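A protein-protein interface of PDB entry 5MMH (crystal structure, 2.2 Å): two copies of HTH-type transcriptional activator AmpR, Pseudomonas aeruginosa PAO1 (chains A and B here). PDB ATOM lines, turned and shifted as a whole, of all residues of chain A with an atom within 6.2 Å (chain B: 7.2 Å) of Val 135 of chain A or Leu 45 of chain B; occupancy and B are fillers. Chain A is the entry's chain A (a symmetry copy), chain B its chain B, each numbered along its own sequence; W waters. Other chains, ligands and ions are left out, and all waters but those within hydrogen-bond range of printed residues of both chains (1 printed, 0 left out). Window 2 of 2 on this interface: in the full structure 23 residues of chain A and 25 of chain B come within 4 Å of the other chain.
The backbone carbonyl oxygen (O) of Leu 45 of chain B lies within hydrogen-bond range of the backbone NH (N) of Val 135 of chain A (3.1 Å). The backbone carbonyl oxygen of Val 135 of chain A sits at hydrogen-bond distance from the backbone NH of Thr 47 of chain B, 3.1 Å away. The side-chain hydroxyl of Thr 47 of chain B sits at hydrogen-bond distance from the side-chain carboxylate of Asp 137 of chain A.
The backbone carbonyl oxygen (O) of Val 16 of chain B is in hydrogen-bond range of the backbone NH (N) of Ser 46 of chain B. The backbone NH (N) of Ala 18 of chain B sits at hydrogen-bond distance from the backbone carbonyl oxygen (O) of Ser 46 of chain B (2.8 Å). The backbone NH (N) of His 48 of chain B lies within hydrogen-bond range of the backbone carbonyl oxygen (O) of Ala 18 of chain B, at 3.2 Å. The backbone carbonyl oxygen (O) of Ile 63 of chain B sits close to a ring nitrogen (NE2) of His 48 of chain B (3.5 Å). The backbone NH (N) of Arg 108 of chain A lies within hydrogen-bond range of the backbone carbonyl oxygen (O) of Ile 134 of chain A, at 3.0 Å. The backbone NH (N) of Phe 136 of chain A lies within hydrogen-bond range of the backbone carbonyl oxygen (O) of Arg 108 of chain A (2.8 Å).
O of Leu 45 of chain B touches CG2 of Ile 134 of chain A, 3.5 Å away. Ser 46 of chain B touches Val 135 of chain A. Phe 136 of chain A touches Thr 47 of chain B (CA to OG1, 3.6 Å). C of His 48 of chain B touches OD2 of Asp 137 of chain A, 3.7 Å away.
Val 135 of chain A touches three residues of chain B. Leu 45 of chain B touches just these residues of chain A: Ile 134 (3.5 Å) and Val 135 (3.1 Å). Printed residues of chain B within 4 Å of Asp 137 of chain A: Thr 47 (2.7 Å) and His 48 (3.7 Å). Of the printed residues of chain A, Thr 47 of chain B touches Val 135 (3.1 Å), Phe 136 (3.6 Å) and Asp 137 (2.7 Å). Of the printed residues of chain B, Ile 134 of chain A touches Leu 45 (3.5 Å). Printed residues of chain B within 4 Å of Phe 136 of chain A: Thr 47 (3.6 Å). The nearest residue of chain B that does not touch Val 135 of chain A is His 48 of chain B (6.3 Å). The nearest residue of chain A that does not touch Leu 45 of chain B is Ser 133 of chain A (4.7 Å). The nearest printed residue of chain A that does not touch Ser 46 of chain B is Ile 134 of chain A (4.9 Å).
Printed residues of chain A that touch a printed residue of chain B: Ile 134, Val 135, Phe 136 and Asp 137. Of the 19 printed residues of chain B, 4 touch a printed residue of chain A. Printed residues of chain B that touch a printed residue of chain A: Leu 45, Ser 46, Thr 47 and His 48. Hydrophobic or aromatic side chains of chain B that line the printed part of chain A: Leu 45. Among the printed residues, 7 pairs touch across the chains.
No position is printed for both chains. Of the 7 pairs that touch across the chains among the printed residues, none has its exchanged pair printed and touching as well.
Water W1 lies within hydrogen-bond range of the side-chain carboxylate (OD1) of Asp 137 of chain A (2.4 Å) and the backbone carbonyl oxygen (O) of His 48 of chain B (3.4 Å).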
ATOM      1  N   LEU A 107       1.427  30.779  17.059  1.00  0.00           N
ATOM      2  CA  LEU A 107       0.656  29.608  16.657  1.00  0.00           C
ATOM      3  C   LEU A 107       0.727  28.559  17.759  1.00  0.00           C
ATOM      4  O   LEU A 107       1.799  28.290  18.302  1.00  0.00           O
ATOM      5  CB  LEU A 107       1.207  29.046  15.352  1.00  0.00           C
ATOM      6  CG  LEU A 107       1.471  30.054  14.230  1.00  0.00           C
ATOM      7  CD1 LEU A 107       2.280  29.400  13.137  1.00  0.00           C
ATOM      8  CD2 LEU A 107       0.128  30.647  13.654  1.00  0.00           C
ATOM      9  N   ARG A 108      -0.413  27.959  18.102  1.00  0.00           N
ATOM     10  CA  ARG A 108      -0.391  27.009  19.203  1.00  0.00           C
ATOM     11  C   ARG A 108      -1.281  25.809  18.922  1.00  0.00           C
ATOM     12  O   ARG A 108      -2.104  25.812  18.005  1.00  0.00           O
ATOM     13  CB  ARG A 108      -0.794  27.683  20.513  1.00  0.00           C
ATOM     14  CG  ARG A 108      -2.224  28.120  20.618  1.00  0.00           C
ATOM     15  CD  ARG A 108      -2.365  28.857  21.934  1.00  0.00           C
ATOM     16  NE  ARG A 108      -3.735  29.203  22.293  1.00  0.00           N
ATOM     17  CZ  ARG A 108      -4.608  28.363  22.844  1.00  0.00           C
ATOM     18  NH1 ARG A 108      -4.278  27.095  23.091  1.00  0.00           N
ATOM     19  NH2 ARG A 108      -5.824  28.797  23.145  1.00  0.00           N
ATOM     20  N   SER A 109      -1.082  24.764  19.727  1.00  0.00           N
ATOM     21  CA  SER A 109      -1.902  23.564  19.716  1.00  0.00           C
ATOM     22  C   SER A 109      -3.015  23.664  20.758  1.00  0.00           C
ATOM     23  O   SER A 109      -3.094  24.624  21.530  1.00  0.00           O
ATOM     24  CB  SER A 109      -1.048  22.327  19.986  1.00  0.00           C
ATOM     25  OG  SER A 109      -0.758  22.226  21.372  1.00  0.00           O
ATOM     26  N   TYR A 110      -3.867  22.640  20.814  1.00  0.00           N
ATOM     27  CA  TYR A 110      -4.939  22.618  21.831  1.00  0.00           C
ATOM     28  C   TYR A 110      -4.467  22.454  23.249  1.00  0.00           C
ATOM     29  O   TYR A 110      -5.201  22.712  24.166  1.00  0.00           O
ATOM     30  CB  TYR A 110      -6.162  21.723  21.572  1.00  0.00           C
ATOM     31  CG  TYR A 110      -6.069  20.577  20.610  1.00  0.00           C
ATOM     32  CD1 TYR A 110      -5.470  19.372  20.977  1.00  0.00           C
ATOM     33  CD2 TYR A 110      -6.669  20.669  19.366  1.00  0.00           C
ATOM     34  CE1 TYR A 110      -5.402  18.301  20.112  1.00  0.00           C
ATOM     35  CE2 TYR A 110      -6.624  19.608  18.464  1.00  0.00           C
ATOM     36  CZ  TYR A 110      -5.975  18.411  18.840  1.00  0.00           C
ATOM     37  OH  TYR A 110      -5.937  17.352  17.951  1.00  0.00           O
ATOM     38  N   ARG A 111      -3.232  22.060  23.422  1.00  0.00           N
ATOM     39  CA  ARG A 111      -2.672  21.994  24.771  1.00  0.00           C
ATOM     40  C   ARG A 111      -2.211  23.392  25.165  1.00  0.00           C
ATOM     41  O   ARG A 111      -1.207  23.891  24.645  1.00  0.00           O
ATOM     42  CB  ARG A 111      -1.527  20.989  24.806  1.00  0.00           C
ATOM     43  CG  ARG A 111      -1.927  19.619  24.298  1.00  0.00           C
ATOM     44  CD  ARG A 111      -0.718  18.706  24.091  1.00  0.00           C
ATOM     45  NE  ARG A 111       0.117  19.128  22.967  1.00  0.00           N
ATOM     46  CZ  ARG A 111      -0.084  18.755  21.704  1.00  0.00           C
ATOM     47  NH1 ARG A 111       0.731  19.188  20.741  1.00  0.00           N
ATOM     48  NH2 ARG A 111      -1.102  17.954  21.403  1.00  0.00           N
ATOM     49  N   SER A 133      -3.649  34.709  18.404  1.00  0.00           N
ATOM     50  CA  SER A 133      -3.194  33.337  18.200  1.00  0.00           C
ATOM     51  C   SER A 133      -4.277  32.475  17.561  1.00  0.00           C
ATOM     52  O   SER A 133      -5.478  32.770  17.621  1.00  0.00           O
ATOM     53  CB  SER A 133      -2.698  32.700  19.512  1.00  0.00           C
ATOM     54  OG  SER A 133      -3.733  32.399  20.430  1.00  0.00           O
ATOM     55  N   ILE A 134      -3.804  31.381  16.962  1.00  0.00           N
ATOM     56  CA  ILE A 134      -4.582  30.445  16.164  1.00  0.00           C
ATOM     57  C   ILE A 134      -4.247  29.060  16.684  1.00  0.00           C
ATOM     58  O   ILE A 134      -3.067  28.740  16.869  1.00  0.00           O
ATOM     59  CB  ILE A 134      -4.217  30.548  14.668  1.00  0.00           C
ATOM     60  CG1 ILE A 134      -4.187  32.012  14.230  1.00  0.00           C
ATOM     61  CG2 ILE A 134      -5.142  29.698  13.815  1.00  0.00           C
ATOM     62  CD1 ILE A 134      -3.370  32.276  12.979  1.00  0.00           C
ATOM     63  N   VAL A 135      -5.261  28.240  16.906  1.00  0.00           N
ATOM     64  CA  VAL A 135      -5.096  26.932  17.536  1.00  0.00           C
ATOM     65  C   VAL A 135      -5.151  25.861  16.458  1.00  0.00           C
ATOM     66  O   VAL A 135      -6.025  25.893  15.580  1.00  0.00           O
ATOM     67  CB  VAL A 135      -6.180  26.686  18.608  1.00  0.00           C
ATOM     68  CG1 VAL A 135      -5.960  25.342  19.287  1.00  0.00           C
ATOM     69  CG2 VAL A 135      -6.196  27.815  19.620  1.00  0.00           C
ATOM     70  N   PHE A 136      -4.240  24.893  16.535  1.00  0.00           N
ATOM     71  CA  PHE A 136      -4.043  23.920  15.471  1.00  0.00           C
ATOM     72  C   PHE A 136      -4.244  22.508  15.994  1.00  0.00           C
ATOM     73  O   PHE A 136      -3.760  22.169  17.075  1.00  0.00           O
ATOM     74  CB  PHE A 136      -2.644  24.060  14.859  1.00  0.00           C
ATOM     75  CG  PHE A 136      -2.499  25.247  13.960  1.00  0.00           C
ATOM     76  CD1 PHE A 136      -2.033  26.458  14.453  1.00  0.00           C
ATOM     77  CD2 PHE A 136      -2.856  25.162  12.625  1.00  0.00           C
ATOM     78  CE1 PHE A 136      -1.910  27.561  13.621  1.00  0.00           C
ATOM     79  CE2 PHE A 136      -2.744  26.253  11.791  1.00  0.00           C
ATOM     80  CZ  PHE A 136      -2.263  27.457  12.285  1.00  0.00           C
ATOM     81  N   ASP A 137      -4.961  21.692  15.223  1.00  0.00           N
ATOM     82  CA  ASP A 137      -5.185  20.310  15.610  1.00  0.00           C
ATOM     83  C   ASP A 137      -3.952  19.460  15.355  1.00  0.00           C
ATOM     84  O   ASP A 137      -3.778  18.435  16.011  1.00  0.00           O
ATOM     85  CB  ASP A 137      -6.405  19.725  14.875  1.00  0.00           C
ATOM     86  CG  ASP A 137      -6.134  19.382  13.364  1.00  0.00           C
ATOM     87  OD1 ASP A 137      -5.622  20.246  12.591  1.00  0.00           O
ATOM     88  OD2 ASP A 137      -6.511  18.249  12.925  1.00  0.00           O
ATOM     89  N   LEU B  14     -15.456  35.853  18.018  1.00  0.00           N
ATOM     90  CA  LEU B  14     -16.024  34.995  16.980  1.00  0.00           C
ATOM     91  C   LEU B  14     -15.152  33.748  16.869  1.00  0.00           C
ATOM     92  O   LEU B  14     -13.949  33.857  16.627  1.00  0.00           O
ATOM     93  CB  LEU B  14     -16.076  35.740  15.650  1.00  0.00           C
ATOM     94  CG  LEU B  14     -16.351  34.970  14.368  1.00  0.00           C
ATOM     95  CD1 LEU B  14     -17.814  34.574  14.251  1.00  0.00           C
ATOM     96  CD2 LEU B  14     -15.903  35.802  13.174  1.00  0.00           C
ATOM     97  N   THR B  15     -15.738  32.574  17.050  1.00  0.00           N
ATOM     98  CA  THR B  15     -14.982  31.327  17.062  1.00  0.00           C
ATOM     99  C   THR B  15     -15.321  30.514  15.814  1.00  0.00           C
ATOM    100  O   THR B  15     -16.444  30.017  15.672  1.00  0.00           O
ATOM    101  CB  THR B  15     -15.272  30.532  18.333  1.00  0.00           C
ATOM    102  OG1 THR B  15     -16.655  30.158  18.349  1.00  0.00           O
ATOM    103  CG2 THR B  15     -14.980  31.382  19.535  1.00  0.00           C
ATOM    104  N   VAL B  16     -14.348  30.375  14.917  1.00  0.00           N
ATOM    105  CA  VAL B  16     -14.506  29.617  13.683  1.00  0.00           C
ATOM    106  C   VAL B  16     -13.585  28.401  13.746  1.00  0.00           C
ATOM    107  O   VAL B  16     -12.386  28.539  14.012  1.00  0.00           O
ATOM    108  CB  VAL B  16     -14.206  30.500  12.458  1.00  0.00           C
ATOM    109  CG1 VAL B  16     -14.239  29.684  11.181  1.00  0.00           C
ATOM    110  CG2 VAL B  16     -15.232  31.657  12.367  1.00  0.00           C
ATOM    111  N   GLY B  17     -14.138  27.220  13.506  1.00  0.00           N
ATOM    112  CA  GLY B  17     -13.330  26.013  13.426  1.00  0.00           C
ATOM    113  C   GLY B  17     -13.302  25.470  12.011  1.00  0.00           C
ATOM    114  O   GLY B  17     -14.321  24.989  11.517  1.00  0.00           O
ATOM    115  N   ALA B  18     -12.163  25.542  11.331  1.00  0.00           N
ATOM    116  CA  ALA B  18     -12.096  25.169   9.924  1.00  0.00           C
ATOM    117  C   ALA B  18     -11.243  23.920   9.758  1.00  0.00           C
ATOM    118  O   ALA B  18     -10.219  23.769  10.433  1.00  0.00           O
ATOM    119  CB  ALA B  18     -11.519  26.317   9.083  1.00  0.00           C
ATOM    120  N   THR B  23      -7.911  25.646   5.907  1.00  0.00           N
ATOM    121  CA  THR B  23      -7.352  26.762   6.666  1.00  0.00           C
ATOM    122  C   THR B  23      -6.014  27.219   6.100  1.00  0.00           C
ATOM    123  O   THR B  23      -5.796  28.409   5.845  1.00  0.00           O
ATOM    124  CB  THR B  23      -7.170  26.332   8.127  1.00  0.00           C
ATOM    125  OG1 THR B  23      -8.403  25.831   8.647  1.00  0.00           O
ATOM    126  CG2 THR B  23      -6.689  27.478   8.989  1.00  0.00           C
ATOM    127  N   LEU B  27      -7.665  29.801   3.466  1.00  0.00           N
ATOM    128  CA  LEU B  27      -8.284  30.814   4.325  1.00  0.00           C
ATOM    129  C   LEU B  27      -7.267  31.746   4.993  1.00  0.00           C
ATOM    130  O   LEU B  27      -7.490  32.966   5.061  1.00  0.00           O
ATOM    131  CB  LEU B  27      -9.158  30.135   5.387  1.00  0.00           C
ATOM    132  CG  LEU B  27      -9.710  31.061   6.474  1.00  0.00           C
ATOM    133  CD1 LEU B  27     -10.746  32.038   5.877  1.00  0.00           C
ATOM    134  CD2 LEU B  27     -10.302  30.281   7.657  1.00  0.00           C
ATOM    135  N   LEU B  28      -6.173  31.204   5.527  1.00  0.00           N
ATOM    136  CA  LEU B  28      -5.177  32.050   6.189  1.00  0.00           C
ATOM    137  C   LEU B  28      -4.524  33.070   5.262  1.00  0.00           C
ATOM    138  O   LEU B  28      -4.295  34.206   5.711  1.00  0.00           O
ATOM    139  CB  LEU B  28      -4.084  31.188   6.848  1.00  0.00           C
ATOM    140  CG  LEU B  28      -4.427  30.404   8.122  1.00  0.00           C
ATOM    141  CD1 LEU B  28      -3.248  29.535   8.601  1.00  0.00           C
ATOM    142  CD2 LEU B  28      -4.871  31.336   9.219  1.00  0.00           C
ATOM    143  N   LEU B  31      -6.917  36.082   5.338  1.00  0.00           N
ATOM    144  CA  LEU B  31      -7.489  36.574   6.585  1.00  0.00           C
ATOM    145  C   LEU B  31      -7.007  37.985   6.922  1.00  0.00           C
ATOM    146  O   LEU B  31      -7.740  38.746   7.568  1.00  0.00           O
ATOM    147  CB  LEU B  31      -7.157  35.595   7.706  1.00  0.00           C
ATOM    148  CG  LEU B  31      -8.227  35.305   8.755  1.00  0.00           C
ATOM    149  CD1 LEU B  31      -9.559  34.890   8.151  1.00  0.00           C
ATOM    150  CD2 LEU B  31      -7.693  34.215   9.658  1.00  0.00           C
ATOM    151  N   ASP B  42     -12.550  39.997  17.266  1.00  0.00           N
ATOM    152  CA  ASP B  42     -11.548  39.090  17.826  1.00  0.00           C
ATOM    153  C   ASP B  42     -11.886  37.687  17.330  1.00  0.00           C
ATOM    154  O   ASP B  42     -12.660  36.955  17.947  1.00  0.00           O
ATOM    155  CB  ASP B  42     -11.522  39.171  19.348  1.00  0.00           C
ATOM    156  CG  ASP B  42     -10.480  38.260  19.968  1.00  0.00           C
ATOM    157  OD1 ASP B  42     -10.671  37.857  21.135  1.00  0.00           O
ATOM    158  OD2 ASP B  42      -9.467  37.954  19.298  1.00  0.00           O
ATOM    159  N   LEU B  43     -11.311  37.325  16.188  1.00  0.00           N
ATOM    160  CA  LEU B  43     -11.485  35.993  15.630  1.00  0.00           C
ATOM    161  C   LEU B  43     -10.639  34.974  16.397  1.00  0.00           C
ATOM    162  O   LEU B  43      -9.441  35.177  16.610  1.00  0.00           O
ATOM    163  CB  LEU B  43     -11.110  35.995  14.146  1.00  0.00           C
ATOM    164  CG  LEU B  43     -11.204  34.651  13.421  1.00  0.00           C
ATOM    165  CD1 LEU B  43     -12.647  34.202  13.378  1.00  0.00           C
ATOM    166  CD2 LEU B  43     -10.604  34.733  12.009  1.00  0.00           C
ATOM    167  N   ARG B  44     -11.274  33.891  16.826  1.00  0.00           N
ATOM    168  CA  ARG B  44     -10.607  32.754  17.451  1.00  0.00           C
ATOM    169  C   ARG B  44     -10.675  31.599  16.459  1.00  0.00           C
ATOM    170  O   ARG B  44     -11.635  30.833  16.441  1.00  0.00           O
ATOM    171  CB  ARG B  44     -11.261  32.378  18.773  1.00  0.00           C
ATOM    172  CG  ARG B  44     -10.491  32.870  19.970  1.00  0.00           C
ATOM    173  CD  ARG B  44     -10.937  34.259  20.266  1.00  0.00           C
ATOM    174  NE  ARG B  44     -10.128  34.937  21.262  1.00  0.00           N
ATOM    175  CZ  ARG B  44     -10.496  35.080  22.528  1.00  0.00           C
ATOM    176  NH1 ARG B  44     -11.645  34.561  22.949  1.00  0.00           N
ATOM    177  NH2 ARG B  44      -9.711  35.731  23.366  1.00  0.00           N
ATOM    178  N   LEU B  45      -9.656  31.484  15.624  1.00  0.00           N
ATOM    179  CA  LEU B  45      -9.627  30.447  14.607  1.00  0.00           C
ATOM    180  C   LEU B  45      -8.991  29.177  15.177  1.00  0.00           C
ATOM    181  O   LEU B  45      -7.947  29.243  15.833  1.00  0.00           O
ATOM    182  CB  LEU B  45      -8.872  30.956  13.378  1.00  0.00           C
ATOM    183  CG  LEU B  45      -8.747  29.958  12.225  1.00  0.00           C
ATOM    184  CD1 LEU B  45     -10.123  29.502  11.666  1.00  0.00           C
ATOM    185  CD2 LEU B  45      -7.869  30.562  11.146  1.00  0.00           C
ATOM    186  N   SER B  46      -9.651  28.033  14.954  1.00  0.00           N
ATOM    187  CA  SER B  46      -9.145  26.708  15.300  1.00  0.00           C
ATOM    188  C   SER B  46      -9.307  25.773  14.101  1.00  0.00           C
ATOM    189  O   SER B  46     -10.152  26.006  13.232  1.00  0.00           O
ATOM    190  CB  SER B  46      -9.868  26.131  16.543  1.00  0.00           C
ATOM    191  OG  SER B  46     -11.243  25.859  16.293  1.00  0.00           O
ATOM    192  N   THR B  47      -8.479  24.718  14.029  1.00  0.00           N
ATOM    193  CA  THR B  47      -8.606  23.742  12.951  1.00  0.00           C
ATOM    194  C   THR B  47      -9.050  22.393  13.498  1.00  0.00           C
ATOM    195  O   THR B  47      -8.992  22.131  14.698  1.00  0.00           O
ATOM    196  CB  THR B  47      -7.310  23.568  12.121  1.00  0.00           C
ATOM    197  OG1 THR B  47      -6.272  22.888  12.861  1.00  0.00           O
ATOM    198  CG2 THR B  47      -6.802  24.908  11.629  1.00  0.00           C
ATOM    199  N   HIS B  48      -9.497  21.537  12.583  1.00  0.00           N
ATOM    200  CA  HIS B  48      -9.986  20.217  12.927  1.00  0.00           C
ATOM    201  C   HIS B  48      -9.812  19.323  11.709  1.00  0.00           C
ATOM    202  O   HIS B  48      -9.340  19.757  10.656  1.00  0.00           O
ATOM    203  CB  HIS B  48     -11.439  20.293  13.424  1.00  0.00           C
ATOM    204  CG  HIS B  48     -12.390  20.948  12.455  1.00  0.00           C
ATOM    205  ND1 HIS B  48     -12.764  20.363  11.263  1.00  0.00           N
ATOM    206  CD2 HIS B  48     -13.071  22.122  12.524  1.00  0.00           C
ATOM    207  CE1 HIS B  48     -13.627  21.148  10.635  1.00  0.00           C
ATOM    208  NE2 HIS B  48     -13.825  22.225  11.374  1.00  0.00           N
ATOM    209  N   LEU B  59     -18.242  26.349  18.818  1.00  0.00           N
ATOM    210  CA  LEU B  59     -17.918  27.214  17.694  1.00  0.00           C
ATOM    211  C   LEU B  59     -19.173  27.949  17.247  1.00  0.00           C
ATOM    212  O   LEU B  59     -20.277  27.407  17.310  1.00  0.00           O
ATOM    213  CB  LEU B  59     -17.340  26.409  16.526  1.00  0.00           C
ATOM    214  CG  LEU B  59     -16.142  25.480  16.760  1.00  0.00           C
ATOM    215  CD1 LEU B  59     -15.926  24.561  15.562  1.00  0.00           C
ATOM    216  CD2 LEU B  59     -14.878  26.286  17.061  1.00  0.00           C
ATOM    217  N   ILE B  63     -16.217  25.228   9.296  1.00  0.00           N
ATOM    218  CA  ILE B  63     -16.037  25.083   7.857  1.00  0.00           C
ATOM    219  C   ILE B  63     -15.656  23.638   7.605  1.00  0.00           C
ATOM    220  O   ILE B  63     -14.642  23.162   8.136  1.00  0.00           O
ATOM    221  CB  ILE B  63     -14.970  26.039   7.304  1.00  0.00           C
ATOM    222  CG1 ILE B  63     -15.494  27.478   7.296  1.00  0.00           C
ATOM    223  CG2 ILE B  63     -14.548  25.613   5.897  1.00  0.00           C
ATOM    224  CD1 ILE B  63     -14.418  28.504   6.996  1.00  0.00           C
ATOM    225  N   PHE B 199     -18.345  38.189   9.224  1.00  0.00           N
ATOM    226  CA  PHE B 199     -17.499  37.120   8.693  1.00  0.00           C
ATOM    227  C   PHE B 199     -18.195  36.390   7.547  1.00  0.00           C
ATOM    228  O   PHE B 199     -17.577  36.106   6.514  1.00  0.00           O
ATOM    229  CB  PHE B 199     -17.104  36.140   9.806  1.00  0.00           C
ATOM    230  CG  PHE B 199     -16.198  35.005   9.339  1.00  0.00           C
ATOM    231  CD1 PHE B 199     -14.867  35.246   9.009  1.00  0.00           C
ATOM    232  CD2 PHE B 199     -16.686  33.707   9.226  1.00  0.00           C
ATOM    233  CE1 PHE B 199     -14.031  34.211   8.571  1.00  0.00           C
ATOM    234  CE2 PHE B 199     -15.866  32.660   8.785  1.00  0.00           C
ATOM    235  CZ  PHE B 199     -14.533  32.919   8.456  1.00  0.00           C
HETATM  236  O   HOH W   1      -5.959  19.362  10.373  1.00  0.00           O
